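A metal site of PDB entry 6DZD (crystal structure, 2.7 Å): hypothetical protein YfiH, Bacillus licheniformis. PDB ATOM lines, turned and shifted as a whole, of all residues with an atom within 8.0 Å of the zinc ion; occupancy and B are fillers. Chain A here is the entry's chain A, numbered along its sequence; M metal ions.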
ATOM      1  N   ASP A 131       5.926  24.226  15.992  1.00  0.00           N
ATOM      2  CA  ASP A 131       5.456  22.971  15.409  1.00  0.00           C
ATOM      3  C   ASP A 131       4.531  23.201  14.201  1.00  0.00           C
ATOM      4  O   ASP A 131       4.612  22.457  13.218  1.00  0.00           O
ATOM      5  CB  ASP A 131       4.709  22.082  16.397  1.00  0.00           C
ATOM      6  CG  ASP A 131       5.619  21.132  17.130  1.00  0.00           C
ATOM      7  OD1 ASP A 131       6.784  20.972  16.701  1.00  0.00           O
ATOM      8  OD2 ASP A 131       5.197  20.561  18.153  1.00  0.00           O
ATOM      9  N   ALA A 185       8.509  22.715  10.474  1.00  0.00           N
ATOM     10  CA  ALA A 185       7.301  22.365  11.209  1.00  0.00           C
ATOM     11  C   ALA A 185       7.423  20.894  11.591  1.00  0.00           C
ATOM     12  O   ALA A 185       8.339  20.184  11.146  1.00  0.00           O
ATOM     13  CB  ALA A 185       6.052  22.657  10.389  1.00  0.00           C
ATOM     14  N   ILE A 186       6.456  20.439  12.397  1.00  0.00           N
ATOM     15  CA  ILE A 186       6.456  19.054  12.877  1.00  0.00           C
ATOM     16  C   ILE A 186       6.185  18.111  11.705  1.00  0.00           C
ATOM     17  O   ILE A 186       5.222  18.270  10.940  1.00  0.00           O
ATOM     18  CB  ILE A 186       5.440  18.881  14.010  1.00  0.00           C
ATOM     19  CG1 ILE A 186       5.581  17.524  14.680  1.00  0.00           C
ATOM     20  CG2 ILE A 186       3.999  19.071  13.542  1.00  0.00           C
ATOM     21  CD1 ILE A 186       4.837  17.448  15.993  1.00  0.00           C
ATOM     22  N   GLY A 187       7.047  17.088  11.564  1.00  0.00           N
ATOM     23  CA  GLY A 187       6.874  16.122  10.492  1.00  0.00           C
ATOM     24  C   GLY A 187       5.868  15.059  10.853  1.00  0.00           C
ATOM     25  O   GLY A 187       5.508  14.897  12.031  1.00  0.00           O
ATOM     26  N   SER A 188       5.419  14.326   9.824  1.00  0.00           N
ATOM     27  CA  SER A 188       4.523  13.209  10.058  1.00  0.00           C
ATOM     28  C   SER A 188       5.193  12.163  10.913  1.00  0.00           C
ATOM     29  O   SER A 188       4.503  11.396  11.599  1.00  0.00           O
ATOM     30  CB  SER A 188       4.031  12.614   8.740  1.00  0.00           C
ATOM     31  OG  SER A 188       5.099  12.118   7.951  1.00  0.00           O
ATOM     32  N   CYS A 189       6.532  12.172  10.960  1.00  0.00           N
ATOM     33  CA  CYS A 189       7.273  11.289  11.845  1.00  0.00           C
ATOM     34  C   CYS A 189       6.827  11.433  13.287  1.00  0.00           C
ATOM     35  O   CYS A 189       6.797  10.447  14.021  1.00  0.00           O
ATOM     36  CB  CYS A 189       8.766  11.589  11.732  1.00  0.00           C
ATOM     37  SG  CYS A 189       9.147  13.342  11.636  1.00  0.00           S
ATOM     38  N   CYS A 190       6.443  12.632  13.724  1.00  0.00           N
ATOM     39  CA  CYS A 190       6.118  12.851  15.130  1.00  0.00           C
ATOM     40  C   CYS A 190       4.692  13.323  15.367  1.00  0.00           C
ATOM     41  O   CYS A 190       4.402  13.753  16.486  1.00  0.00           O
ATOM     42  CB  CYS A 190       7.056  13.884  15.773  1.00  0.00           C
ATOM     43  SG  CYS A 190       8.759  13.867  15.210  1.00  0.00           S
ATOM     44  N   TYR A 191       3.807  13.291  14.379  1.00  0.00           N
ATOM     45  CA  TYR A 191       2.494  13.945  14.508  1.00  0.00           C
ATOM     46  C   TYR A 191       1.359  12.970  14.210  1.00  0.00           C
ATOM     47  O   TYR A 191       1.187  12.532  13.063  1.00  0.00           O
ATOM     48  CB  TYR A 191       2.417  15.154  13.581  1.00  0.00           C
ATOM     49  CG  TYR A 191       1.204  16.020  13.830  1.00  0.00           C
ATOM     50  CD1 TYR A 191       0.861  16.405  15.129  1.00  0.00           C
ATOM     51  CD2 TYR A 191       0.393  16.460  12.776  1.00  0.00           C
ATOM     52  CE1 TYR A 191      -0.250  17.203  15.358  1.00  0.00           C
ATOM     53  CE2 TYR A 191      -0.723  17.254  13.013  1.00  0.00           C
ATOM     54  CZ  TYR A 191      -1.035  17.626  14.310  1.00  0.00           C
ATOM     55  OH  TYR A 191      -2.142  18.413  14.575  1.00  0.00           O
ATOM     56  N   ARG A 222      -1.336   9.226  11.091  1.00  0.00           N
ATOM     57  CA  ARG A 222      -0.122   9.997  10.863  1.00  0.00           C
ATOM     58  C   ARG A 222      -0.446  11.035   9.803  1.00  0.00           C
ATOM     59  O   ARG A 222      -1.124  10.731   8.812  1.00  0.00           O
ATOM     60  CB  ARG A 222       0.975   9.061  10.373  1.00  0.00           C
ATOM     61  CG  ARG A 222       2.356   9.452  10.747  1.00  0.00           C
ATOM     62  CD  ARG A 222       3.242   8.218  10.890  1.00  0.00           C
ATOM     63  NE  ARG A 222       3.133   7.585  12.206  1.00  0.00           N
ATOM     64  CZ  ARG A 222       3.549   8.115  13.366  1.00  0.00           C
ATOM     65  NH1 ARG A 222       4.115   9.322  13.413  1.00  0.00           N
ATOM     66  NH2 ARG A 222       3.416   7.441  14.493  1.00  0.00           N
ATOM     67  N   SER A 247      12.831  20.272   4.960  1.00  0.00           N
ATOM     68  CA  SER A 247      12.670  18.938   5.507  1.00  0.00           C
ATOM     69  C   SER A 247      12.785  18.906   7.030  1.00  0.00           C
ATOM     70  O   SER A 247      12.480  17.861   7.632  1.00  0.00           O
ATOM     71  CB  SER A 247      13.701  18.000   4.894  1.00  0.00           C
ATOM     72  OG  SER A 247      14.994  18.536   5.130  1.00  0.00           O
ATOM     73  N   LEU A 248      13.100  20.040   7.667  1.00  0.00           N
ATOM     74  CA  LEU A 248      13.366  20.059   9.089  1.00  0.00           C
ATOM     75  C   LEU A 248      12.085  19.843   9.890  1.00  0.00           C
ATOM     76  O   LEU A 248      11.051  20.463   9.620  1.00  0.00           O
ATOM     77  CB  LEU A 248      14.027  21.378   9.497  1.00  0.00           C
ATOM     78  CG  LEU A 248      15.462  21.603   8.948  1.00  0.00           C
ATOM     79  CD1 LEU A 248      15.960  22.990   9.338  1.00  0.00           C
ATOM     80  CD2 LEU A 248      16.455  20.537   9.402  1.00  0.00           C
ATOM     81  N   CYS A 249      12.145  18.933  10.851  1.00  0.00           N
ATOM     82  CA  CYS A 249      11.056  18.646  11.769  1.00  0.00           C
ATOM     83  C   CYS A 249      11.342  19.348  13.106  1.00  0.00           C
ATOM     84  O   CYS A 249      12.407  19.142  13.703  1.00  0.00           O
ATOM     85  CB  CYS A 249      10.902  17.144  11.955  1.00  0.00           C
ATOM     86  SG  CYS A 249       9.653  16.665  13.147  1.00  0.00           S
ATOM     87  N   THR A 250      10.411  20.168  13.558  1.00  0.00           N
ATOM     88  CA  THR A 250      10.644  20.907  14.791  1.00  0.00           C
ATOM     89  C   THR A 250      10.717  19.970  15.999  1.00  0.00           C
ATOM     90  O   THR A 250      11.455  20.249  16.958  1.00  0.00           O
ATOM     91  CB  THR A 250       9.587  22.006  14.979  1.00  0.00           C
ATOM     92  OG1 THR A 250       8.271  21.439  14.964  1.00  0.00           O
ATOM     93  CG2 THR A 250       9.695  23.027  13.872  1.00  0.00           C
ATOM     94  N   SER A 251       9.968  18.865  15.970  1.00  0.00           N
ATOM     95  CA  SER A 251      10.062  17.886  17.043  1.00  0.00           C
ATOM     96  C   SER A 251      11.415  17.167  17.032  1.00  0.00           C
ATOM     97  O   SER A 251      12.042  16.994  18.087  1.00  0.00           O
ATOM     98  CB  SER A 251       8.920  16.869  16.915  1.00  0.00           C
ATOM     99  OG  SER A 251       8.996  15.862  17.905  1.00  0.00           O
ATOM    100  N   CYS A 252      11.882  16.742  15.853  1.00  0.00           N
ATOM    101  CA  CYS A 252      13.096  15.951  15.802  1.00  0.00           C
ATOM    102  C   CYS A 252      14.332  16.771  16.145  1.00  0.00           C
ATOM    103  O   CYS A 252      15.205  16.294  16.877  1.00  0.00           O
ATOM    104  CB  CYS A 252      13.250  15.337  14.410  1.00  0.00           C
ATOM    105  SG  CYS A 252      12.201  13.921  14.111  1.00  0.00           S
ATOM    106  N   GLU A 253      14.419  18.004  15.661  1.00  0.00           N
ATOM    107  CA  GLU A 253      15.644  18.797  15.764  1.00  0.00           C
ATOM    108  C   GLU A 253      15.697  19.429  17.151  1.00  0.00           C
ATOM    109  O   GLU A 253      15.322  20.592  17.354  1.00  0.00           O
ATOM    110  CB  GLU A 253      15.707  19.845  14.660  1.00  0.00           C
ATOM    111  CG  GLU A 253      15.542  19.317  13.215  1.00  0.00           C
ATOM    112  CD  GLU A 253      16.686  18.408  12.801  1.00  0.00           C
ATOM    113  OE1 GLU A 253      16.567  17.726  11.745  1.00  0.00           O
ATOM    114  OE2 GLU A 253      17.695  18.375  13.541  1.00  0.00           O
ATOM    115  N   SER A 259       9.415  22.748  20.288  1.00  0.00           N
ATOM    116  CA  SER A 259       8.355  21.912  19.736  1.00  0.00           C
ATOM    117  C   SER A 259       7.250  21.743  20.760  1.00  0.00           C
ATOM    118  O   SER A 259       7.501  21.239  21.862  1.00  0.00           O
ATOM    119  CB  SER A 259       8.874  20.551  19.307  1.00  0.00           C
ATOM    120  OG  SER A 259       7.780  19.726  18.983  1.00  0.00           O
HETATM  121 ZN    ZN M   1       9.988  14.433  13.509  1.00  0.00          ZN
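Of the 17 residues printed, 4 come within 4 Å of the zinc ion.
The nearest printed residue that does not touch the zinc ion is Ser 251 (4.3 Å).
The side-chain sulfur (SG) of Cys 190 lies close to the side-chain hydroxyl (OG) of Ser 251 (3.4 Å).
The side-chain sulfur of Cys 249 sits close to the backbone NH of Ser 251.
The backbone NH (N) of Gly 187 lies close to the side-chain sulfur (SG) of Cys 249.
The backbone carbonyl oxygen (O) of Cys 189 lies within hydrogen-bond range of the guanidinium group (NH1) of Arg 222.
The zinc ion is bound by SG of Cys 190, SG of Cys 249, SG of Cys 189 and SG of Cys 252.
The zinc ion has four donor atoms within binding distance.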
